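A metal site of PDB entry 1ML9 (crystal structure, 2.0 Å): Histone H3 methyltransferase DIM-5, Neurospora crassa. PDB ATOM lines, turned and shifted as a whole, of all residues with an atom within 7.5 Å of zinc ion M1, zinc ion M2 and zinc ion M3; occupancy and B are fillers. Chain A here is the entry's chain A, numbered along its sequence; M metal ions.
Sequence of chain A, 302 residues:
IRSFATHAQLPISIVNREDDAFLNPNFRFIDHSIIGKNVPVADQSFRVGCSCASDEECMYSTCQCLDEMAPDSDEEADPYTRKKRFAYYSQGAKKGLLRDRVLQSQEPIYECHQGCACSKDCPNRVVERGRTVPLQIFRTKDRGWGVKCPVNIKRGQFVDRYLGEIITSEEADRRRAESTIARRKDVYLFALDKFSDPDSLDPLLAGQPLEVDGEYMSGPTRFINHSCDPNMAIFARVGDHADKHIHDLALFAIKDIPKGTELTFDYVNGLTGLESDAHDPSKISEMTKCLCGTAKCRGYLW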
ATOM      1  N   VAL A  48     -19.052 -27.560 -23.745  1.00  0.00           N
ATOM      2  CA  VAL A  48     -18.168 -26.436 -23.514  1.00  0.00           C
ATOM      3  C   VAL A  48     -18.870 -25.317 -22.727  1.00  0.00           C
ATOM      4  O   VAL A  48     -20.036 -24.987 -22.984  1.00  0.00           O
ATOM      5  CB  VAL A  48     -17.584 -25.889 -24.888  1.00  0.00           C
ATOM      6  CG1 VAL A  48     -18.498 -26.256 -26.040  1.00  0.00           C
ATOM      7  CG2 VAL A  48     -17.377 -24.385 -24.841  1.00  0.00           C
ATOM      8  N   GLY A  49     -18.157 -24.763 -21.742  1.00  0.00           N
ATOM      9  CA  GLY A  49     -18.687 -23.675 -20.942  1.00  0.00           C
ATOM     10  C   GLY A  49     -17.860 -22.423 -21.201  1.00  0.00           C
ATOM     11  O   GLY A  49     -16.699 -22.539 -21.590  1.00  0.00           O
ATOM     12  N   CYS A  50     -18.437 -21.237 -21.014  1.00  0.00           N
ATOM     13  CA  CYS A  50     -17.696 -19.999 -21.249  1.00  0.00           C
ATOM     14  C   CYS A  50     -16.574 -19.875 -20.226  1.00  0.00           C
ATOM     15  O   CYS A  50     -16.626 -20.494 -19.168  1.00  0.00           O
ATOM     16  CB  CYS A  50     -18.623 -18.790 -21.169  1.00  0.00           C
ATOM     17  SG  CYS A  50     -19.322 -18.441 -19.518  1.00  0.00           S
ATOM     18  N   SER A  51     -15.564 -19.069 -20.556  1.00  0.00           N
ATOM     19  CA  SER A  51     -14.428 -18.884 -19.658  1.00  0.00           C
ATOM     20  C   SER A  51     -14.382 -17.480 -19.070  1.00  0.00           C
ATOM     21  O   SER A  51     -13.319 -16.964 -18.739  1.00  0.00           O
ATOM     22  CB  SER A  51     -13.116 -19.153 -20.414  1.00  0.00           C
ATOM     23  OG  SER A  51     -13.004 -18.310 -21.542  1.00  0.00           O
ATOM     24  N   CYS A  52     -15.555 -16.872 -18.922  1.00  0.00           N
ATOM     25  CA  CYS A  52     -15.656 -15.523 -18.376  1.00  0.00           C
ATOM     26  C   CYS A  52     -14.958 -15.365 -17.035  1.00  0.00           C
ATOM     27  O   CYS A  52     -15.074 -16.218 -16.148  1.00  0.00           O
ATOM     28  CB  CYS A  52     -17.116 -15.126 -18.265  1.00  0.00           C
ATOM     29  SG  CYS A  52     -17.859 -14.751 -19.883  1.00  0.00           S
ATOM     30  N   ALA A  53     -14.213 -14.257 -16.899  1.00  0.00           N
ATOM     31  CA  ALA A  53     -13.487 -13.979 -15.683  1.00  0.00           C
ATOM     32  C   ALA A  53     -14.390 -13.877 -14.469  1.00  0.00           C
ATOM     33  O   ALA A  53     -14.135 -14.511 -13.442  1.00  0.00           O
ATOM     34  N   SER A  54     -15.443 -13.064 -14.581  1.00  0.00           N
ATOM     35  CA  SER A  54     -16.390 -12.891 -13.488  1.00  0.00           C
ATOM     36  C   SER A  54     -17.825 -12.973 -14.009  1.00  0.00           C
ATOM     37  O   SER A  54     -18.080 -12.686 -15.180  1.00  0.00           O
ATOM     38  CB  SER A  54     -16.161 -11.549 -12.802  1.00  0.00           C
ATOM     39  N   ASP A  55     -18.737 -13.366 -13.126  1.00  0.00           N
ATOM     40  CA  ASP A  55     -20.146 -13.492 -13.460  1.00  0.00           C
ATOM     41  C   ASP A  55     -20.675 -12.280 -14.209  1.00  0.00           C
ATOM     42  O   ASP A  55     -21.723 -12.341 -14.848  1.00  0.00           O
ATOM     43  CB  ASP A  55     -20.971 -13.693 -12.182  1.00  0.00           C
ATOM     44  CG  ASP A  55     -20.672 -15.004 -11.520  1.00  0.00           C
ATOM     45  OD1 ASP A  55     -19.643 -15.612 -11.875  1.00  0.00           O
ATOM     46  OD2 ASP A  55     -21.472 -15.450 -10.664  1.00  0.00           O
ATOM     47  N   GLU A  56     -19.951 -11.168 -14.142  1.00  0.00           N
ATOM     48  CA  GLU A  56     -20.370  -9.947 -14.803  1.00  0.00           C
ATOM     49  C   GLU A  56     -20.108  -9.949 -16.315  1.00  0.00           C
ATOM     50  O   GLU A  56     -20.912  -9.403 -17.081  1.00  0.00           O
ATOM     51  CB  GLU A  56     -19.696  -8.752 -14.153  1.00  0.00           C
ATOM     52  N   GLU A  57     -19.001 -10.546 -16.751  1.00  0.00           N
ATOM     53  CA  GLU A  57     -18.687 -10.572 -18.175  1.00  0.00           C
ATOM     54  C   GLU A  57     -19.679 -11.346 -19.034  1.00  0.00           C
ATOM     55  O   GLU A  57     -19.886 -11.035 -20.215  1.00  0.00           O
ATOM     56  N   CYS A  58     -20.305 -12.357 -18.432  1.00  0.00           N
ATOM     57  CA  CYS A  58     -21.260 -13.203 -19.117  1.00  0.00           C
ATOM     58  C   CYS A  58     -22.435 -12.479 -19.783  1.00  0.00           C
ATOM     59  O   CYS A  58     -23.104 -13.060 -20.640  1.00  0.00           O
ATOM     60  CB  CYS A  58     -21.817 -14.251 -18.149  1.00  0.00           C
ATOM     61  SG  CYS A  58     -20.617 -15.536 -17.663  1.00  0.00           S
ATOM     62  N   MET A  59     -22.691 -11.230 -19.408  1.00  0.00           N
ATOM     63  CA  MET A  59     -23.809 -10.510 -20.028  1.00  0.00           C
ATOM     64  C   MET A  59     -23.409  -9.717 -21.251  1.00  0.00           C
ATOM     65  O   MET A  59     -24.213  -8.962 -21.803  1.00  0.00           O
ATOM     66  CB  MET A  59     -24.502  -9.585 -19.024  1.00  0.00           C
ATOM     67  CG  MET A  59     -23.631  -9.015 -17.934  1.00  0.00           C
ATOM     68  SD  MET A  59     -24.605  -8.075 -16.734  1.00  0.00           S
ATOM     69  CE  MET A  59     -23.930  -8.689 -15.174  1.00  0.00           C
ATOM     70  N   TYR A  60     -22.169  -9.898 -21.701  1.00  0.00           N
ATOM     71  CA  TYR A  60     -21.667  -9.187 -22.876  1.00  0.00           C
ATOM     72  C   TYR A  60     -21.456 -10.098 -24.086  1.00  0.00           C
ATOM     73  O   TYR A  60     -21.332 -11.323 -23.964  1.00  0.00           O
ATOM     74  CB  TYR A  60     -20.371  -8.465 -22.530  1.00  0.00           C
ATOM     75  CG  TYR A  60     -20.551  -7.359 -21.520  1.00  0.00           C
ATOM     76  CD1 TYR A  60     -20.125  -7.526 -20.199  1.00  0.00           C
ATOM     77  CD2 TYR A  60     -21.139  -6.149 -21.882  1.00  0.00           C
ATOM     78  CE1 TYR A  60     -20.291  -6.503 -19.265  1.00  0.00           C
ATOM     79  CE2 TYR A  60     -21.312  -5.123 -20.955  1.00  0.00           C
ATOM     80  CZ  TYR A  60     -20.879  -5.312 -19.639  1.00  0.00           C
ATOM     81  OH  TYR A  60     -21.025  -4.297 -18.717  1.00  0.00           O
ATOM     82  N   THR A  62     -19.097 -10.927 -25.557  1.00  0.00           N
ATOM     83  CA  THR A  62     -17.867 -11.706 -25.496  1.00  0.00           C
ATOM     84  C   THR A  62     -18.019 -13.039 -24.788  1.00  0.00           C
ATOM     85  O   THR A  62     -17.125 -13.893 -24.842  1.00  0.00           O
ATOM     86  CB  THR A  62     -16.748 -10.923 -24.790  1.00  0.00           C
ATOM     87  OG1 THR A  62     -16.923 -11.017 -23.365  1.00  0.00           O
ATOM     88  CG2 THR A  62     -16.768  -9.463 -25.203  1.00  0.00           C
ATOM     89  N   CYS A  63     -19.133 -13.243 -24.102  1.00  0.00           N
ATOM     90  CA  CYS A  63     -19.347 -14.504 -23.413  1.00  0.00           C
ATOM     91  C   CYS A  63     -19.514 -15.586 -24.487  1.00  0.00           C
ATOM     92  O   CYS A  63     -20.267 -15.410 -25.452  1.00  0.00           O
ATOM     93  CB  CYS A  63     -20.584 -14.410 -22.520  1.00  0.00           C
ATOM     94  SG  CYS A  63     -21.025 -15.964 -21.675  1.00  0.00           S
ATOM     95  N   GLN A  64     -18.798 -16.697 -24.324  1.00  0.00           N
ATOM     96  CA  GLN A  64     -18.875 -17.808 -25.275  1.00  0.00           C
ATOM     97  C   GLN A  64     -20.289 -18.319 -25.450  1.00  0.00           C
ATOM     98  O   GLN A  64     -20.715 -18.656 -26.554  1.00  0.00           O
ATOM     99  CB  GLN A  64     -17.989 -18.965 -24.798  1.00  0.00           C
ATOM    100  CG  GLN A  64     -16.606 -18.957 -25.399  1.00  0.00           C
ATOM    101  CD  GLN A  64     -15.565 -18.418 -24.437  1.00  0.00           C
ATOM    102  OE1 GLN A  64     -15.826 -18.242 -23.246  1.00  0.00           O
ATOM    103  NE2 GLN A  64     -14.362 -18.142 -24.958  1.00  0.00           N
ATOM    104  N   CYS A  65     -21.016 -18.369 -24.343  1.00  0.00           N
ATOM    105  CA  CYS A  65     -22.391 -18.848 -24.319  1.00  0.00           C
ATOM    106  C   CYS A  65     -23.329 -18.096 -25.236  1.00  0.00           C
ATOM    107  O   CYS A  65     -24.256 -18.670 -25.799  1.00  0.00           O
ATOM    108  CB  CYS A  65     -22.899 -18.816 -22.882  1.00  0.00           C
ATOM    109  SG  CYS A  65     -22.039 -20.058 -21.880  1.00  0.00           S
ATOM    110  N   LEU A  66     -23.070 -16.800 -25.394  1.00  0.00           N
ATOM    111  CA  LEU A  66     -23.917 -15.975 -26.244  1.00  0.00           C
ATOM    112  C   LEU A  66     -23.377 -15.919 -27.667  1.00  0.00           C
ATOM    113  O   LEU A  66     -23.867 -15.143 -28.495  1.00  0.00           O
ATOM    114  CB  LEU A  66     -24.017 -14.577 -25.639  1.00  0.00           C
ATOM    115  CG  LEU A  66     -24.734 -14.429 -24.289  1.00  0.00           C
ATOM    116  CD1 LEU A  66     -23.982 -15.133 -23.170  1.00  0.00           C
ATOM    117  CD2 LEU A  66     -24.844 -12.946 -23.978  1.00  0.00           C
ATOM    118  N   TYR A 110     -30.066 -18.276 -24.644  1.00  0.00           N
ATOM    119  CA  TYR A 110     -28.794 -18.964 -24.403  1.00  0.00           C
ATOM    120  C   TYR A 110     -28.257 -18.596 -23.021  1.00  0.00           C
ATOM    121  O   TYR A 110     -27.815 -17.455 -22.798  1.00  0.00           O
ATOM    122  CB  TYR A 110     -27.788 -18.581 -25.493  1.00  0.00           C
ATOM    123  CG  TYR A 110     -28.135 -19.166 -26.840  1.00  0.00           C
ATOM    124  CD1 TYR A 110     -28.897 -18.452 -27.751  1.00  0.00           C
ATOM    125  CD2 TYR A 110     -27.723 -20.454 -27.189  1.00  0.00           C
ATOM    126  CE1 TYR A 110     -29.248 -18.989 -28.987  1.00  0.00           C
ATOM    127  CE2 TYR A 110     -28.072 -21.013 -28.407  1.00  0.00           C
ATOM    128  CZ  TYR A 110     -28.829 -20.273 -29.309  1.00  0.00           C
ATOM    129  OH  TYR A 110     -29.170 -20.810 -30.525  1.00  0.00           O
ATOM    130  N   GLU A 111     -28.302 -19.555 -22.111  1.00  0.00           N
ATOM    131  CA  GLU A 111     -27.862 -19.370 -20.738  1.00  0.00           C
ATOM    132  C   GLU A 111     -26.555 -20.069 -20.415  1.00  0.00           C
ATOM    133  O   GLU A 111     -26.054 -20.881 -21.205  1.00  0.00           O
ATOM    134  CB  GLU A 111     -28.925 -19.919 -19.774  1.00  0.00           C
ATOM    135  CG  GLU A 111     -30.151 -19.056 -19.584  1.00  0.00           C
ATOM    136  CD  GLU A 111     -30.876 -19.380 -18.295  1.00  0.00           C
ATOM    137  OE1 GLU A 111     -31.745 -18.575 -17.898  1.00  0.00           O
ATOM    138  OE2 GLU A 111     -30.593 -20.417 -17.670  1.00  0.00           O
ATOM    139  N   CYS A 112     -26.003 -19.747 -19.251  1.00  0.00           N
ATOM    140  CA  CYS A 112     -24.792 -20.397 -18.807  1.00  0.00           C
ATOM    141  C   CYS A 112     -25.268 -21.735 -18.252  1.00  0.00           C
ATOM    142  O   CYS A 112     -26.482 -21.958 -18.138  1.00  0.00           O
ATOM    143  CB  CYS A 112     -24.074 -19.558 -17.749  1.00  0.00           C
ATOM    144  SG  CYS A 112     -23.043 -18.265 -18.536  1.00  0.00           S
ATOM    145  N   HIS A 113     -24.350 -22.628 -17.905  1.00  0.00           N
ATOM    146  CA  HIS A 113     -24.768 -23.953 -17.471  1.00  0.00           C
ATOM    147  C   HIS A 113     -23.632 -24.708 -16.827  1.00  0.00           C
ATOM    148  O   HIS A 113     -22.543 -24.151 -16.613  1.00  0.00           O
ATOM    149  CB  HIS A 113     -25.194 -24.721 -18.721  1.00  0.00           C
ATOM    150  CG  HIS A 113     -24.284 -24.491 -19.885  1.00  0.00           C
ATOM    151  ND1 HIS A 113     -24.388 -23.381 -20.702  1.00  0.00           N
ATOM    152  CD2 HIS A 113     -23.186 -25.155 -20.299  1.00  0.00           C
ATOM    153  CE1 HIS A 113     -23.397 -23.380 -21.572  1.00  0.00           C
ATOM    154  NE2 HIS A 113     -22.655 -24.446 -21.348  1.00  0.00           N
ATOM    155  N   GLY A 115     -20.515 -26.230 -16.346  1.00  0.00           N
ATOM    156  CA  GLY A 115     -19.332 -26.125 -17.165  1.00  0.00           C
ATOM    157  C   GLY A 115     -18.743 -24.734 -17.240  1.00  0.00           C
ATOM    158  O   GLY A 115     -17.524 -24.584 -17.321  1.00  0.00           O
ATOM    159  N   CYS A 116     -19.597 -23.715 -17.204  1.00  0.00           N
ATOM    160  CA  CYS A 116     -19.114 -22.337 -17.264  1.00  0.00           C
ATOM    161  C   CYS A 116     -18.238 -21.952 -16.076  1.00  0.00           C
ATOM    162  O   CYS A 116     -18.419 -22.455 -14.969  1.00  0.00           O
ATOM    163  CB  CYS A 116     -20.289 -21.374 -17.365  1.00  0.00           C
ATOM    164  SG  CYS A 116     -21.178 -21.541 -18.930  1.00  0.00           S
ATOM    165  N   ALA A 117     -17.309 -21.033 -16.331  1.00  0.00           N
ATOM    166  CA  ALA A 117     -16.372 -20.550 -15.318  1.00  0.00           C
ATOM    167  C   ALA A 117     -17.004 -19.542 -14.351  1.00  0.00           C
ATOM    168  O   ALA A 117     -16.334 -19.027 -13.452  1.00  0.00           O
ATOM    169  CB  ALA A 117     -15.154 -19.923 -15.995  1.00  0.00           C
ATOM    170  N   CYS A 118     -18.283 -19.249 -14.564  1.00  0.00           N
ATOM    171  CA  CYS A 118     -18.990 -18.314 -13.699  1.00  0.00           C
ATOM    172  C   CYS A 118     -19.607 -19.118 -12.558  1.00  0.00           C
ATOM    173  O   CYS A 118     -19.541 -20.354 -12.553  1.00  0.00           O
ATOM    174  CB  CYS A 118     -20.067 -17.584 -14.487  1.00  0.00           C
ATOM    175  SG  CYS A 118     -21.205 -18.687 -15.382  1.00  0.00           S
ATOM    176  N   SER A 119     -20.208 -18.426 -11.595  1.00  0.00           N
ATOM    177  CA  SER A 119     -20.820 -19.105 -10.471  1.00  0.00           C
ATOM    178  C   SER A 119     -22.317 -19.255 -10.608  1.00  0.00           C
ATOM    179  O   SER A 119     -22.929 -18.643 -11.487  1.00  0.00           O
ATOM    180  N   ASP A 121     -24.388 -17.940  -9.268  1.00  0.00           N
ATOM    181  CA  ASP A 121     -24.945 -16.602  -9.209  1.00  0.00           C
ATOM    182  C   ASP A 121     -24.897 -15.832 -10.516  1.00  0.00           C
ATOM    183  O   ASP A 121     -25.306 -14.677 -10.566  1.00  0.00           O
ATOM    184  CB  ASP A 121     -24.231 -15.802  -8.121  1.00  0.00           C
ATOM    185  N   CYS A 122     -24.394 -16.464 -11.576  1.00  0.00           N
ATOM    186  CA  CYS A 122     -24.300 -15.793 -12.862  1.00  0.00           C
ATOM    187  C   CYS A 122     -25.650 -15.214 -13.301  1.00  0.00           C
ATOM    188  O   CYS A 122     -26.652 -15.920 -13.325  1.00  0.00           O
ATOM    189  CB  CYS A 122     -23.783 -16.748 -13.942  1.00  0.00           C
ATOM    190  SG  CYS A 122     -23.787 -15.989 -15.596  1.00  0.00           S
ATOM    191  N   PRO A 123     -25.668 -13.929 -13.668  1.00  0.00           N
ATOM    192  CA  PRO A 123     -26.906 -13.266 -14.107  1.00  0.00           C
ATOM    193  C   PRO A 123     -27.575 -13.952 -15.294  1.00  0.00           C
ATOM    194  O   PRO A 123     -28.708 -13.630 -15.639  1.00  0.00           O
ATOM    195  CB  PRO A 123     -26.455 -11.840 -14.457  1.00  0.00           C
ATOM    196  CG  PRO A 123     -24.965 -11.910 -14.612  1.00  0.00           C
ATOM    197  CD  PRO A 123     -24.511 -13.014 -13.685  1.00  0.00           C
ATOM    198  N   ASN A 124     -26.857 -14.880 -15.911  1.00  0.00           N
ATOM    199  CA  ASN A 124     -27.391 -15.587 -17.070  1.00  0.00           C
ATOM    200  C   ASN A 124     -27.658 -17.045 -16.784  1.00  0.00           C
ATOM    201  O   ASN A 124     -27.426 -17.908 -17.622  1.00  0.00           O
ATOM    202  CB  ASN A 124     -26.433 -15.461 -18.250  1.00  0.00           C
ATOM    203  CG  ASN A 124     -27.111 -15.738 -19.568  1.00  0.00           C
ATOM    204  OD1 ASN A 124     -28.264 -15.368 -19.768  1.00  0.00           O
ATOM    205  ND2 ASN A 124     -26.403 -16.402 -20.475  1.00  0.00           N
ATOM    206  N   ARG A 125     -28.164 -17.316 -15.583  1.00  0.00           N
ATOM    207  CA  ARG A 125     -28.508 -18.672 -15.170  1.00  0.00           C
ATOM    208  C   ARG A 125     -29.879 -18.650 -14.503  1.00  0.00           C
ATOM    209  O   ARG A 125     -30.205 -19.527 -13.713  1.00  0.00           O
ATOM    210  CB  ARG A 125     -27.473 -19.216 -14.182  1.00  0.00           C
ATOM    211  CG  ARG A 125     -26.100 -19.498 -14.772  1.00  0.00           C
ATOM    212  CD  ARG A 125     -25.111 -19.912 -13.692  1.00  0.00           C
ATOM    213  NE  ARG A 125     -23.781 -20.175 -14.224  1.00  0.00           N
ATOM    214  CZ  ARG A 125     -23.187 -21.372 -14.228  1.00  0.00           C
ATOM    215  NH1 ARG A 125     -23.809 -22.431 -13.737  1.00  0.00           N
ATOM    216  NH2 ARG A 125     -21.964 -21.502 -14.726  1.00  0.00           N
HETATM  217 ZN    ZN M   1     -19.718 -16.154 -19.768  1.00  0.00          ZN
HETATM  218 ZN    ZN M   2     -21.409 -19.476 -19.760  1.00  0.00          ZN
HETATM  219 ZN    ZN M   3     -22.089 -17.099 -16.774  1.00  0.00          ZN
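N of Asn 124 lies close to SG of Cys 122 (3.3 Å).
The backbone NH of Cys 65 lies close to the side-chain sulfur of Cys 63, at 3.6 Å.
NH2 of Arg 125 is in hydrogen-bond range of O of Cys 118 (3.5 Å).
N of Cys 112 lies within hydrogen-bond range of O of Asn 124, at 2.8 Å.
The backbone carbonyl oxygen of Cys 50 sits at hydrogen-bond distance from the backbone NH of Ala 117, 3.0 Å away.
OD2 of Asp 55 sits at hydrogen-bond distance from N of Cys 122.
The side-chain sulfur of Cys 116 sits close to the backbone NH of His 113, 3.5 Å away.
The nearest printed residue that does not touch zinc ion M1 is Cys 112 (4.1 Å).
The nearest printed residue that does not touch zinc ion M2 is Cys 63 (4.02 Å).
Four residues have an atom within 4 Å of zinc ion M3: Cys 58, Cys 112, Cys 118 and Cys 122.
The nearest printed residue that does not touch zinc ion M3 is Cys 50 (4.1 Å).
Zinc ion M1 is bound by SG of Cys 63 (2.3 Å), SG of Cys 52 (2.3 Å), SG of Cys 50 (2.3 Å) and SG of Cys 58 (2.4 Å).
Zinc ion M1 has four donor atoms within binding distance.
Zinc ion M2 is bound by SG of Cys 116 (2.2 Å), SG of Cys 65 (2.3 Å), SG of Cys 50 (2.3 Å) and SG of Cys 112 (2.4 Å).
Zinc ion M2 has four donor atoms within binding distance.
Zinc ion M3 is bound by SG of Cys 118 (2.3 Å), SG of Cys 112 (2.3 Å), SG of Cys 58 (2.3 Å) and SG of Cys 122 (2.3 Å).
Zinc ion M3 has four donor atoms within binding distance.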
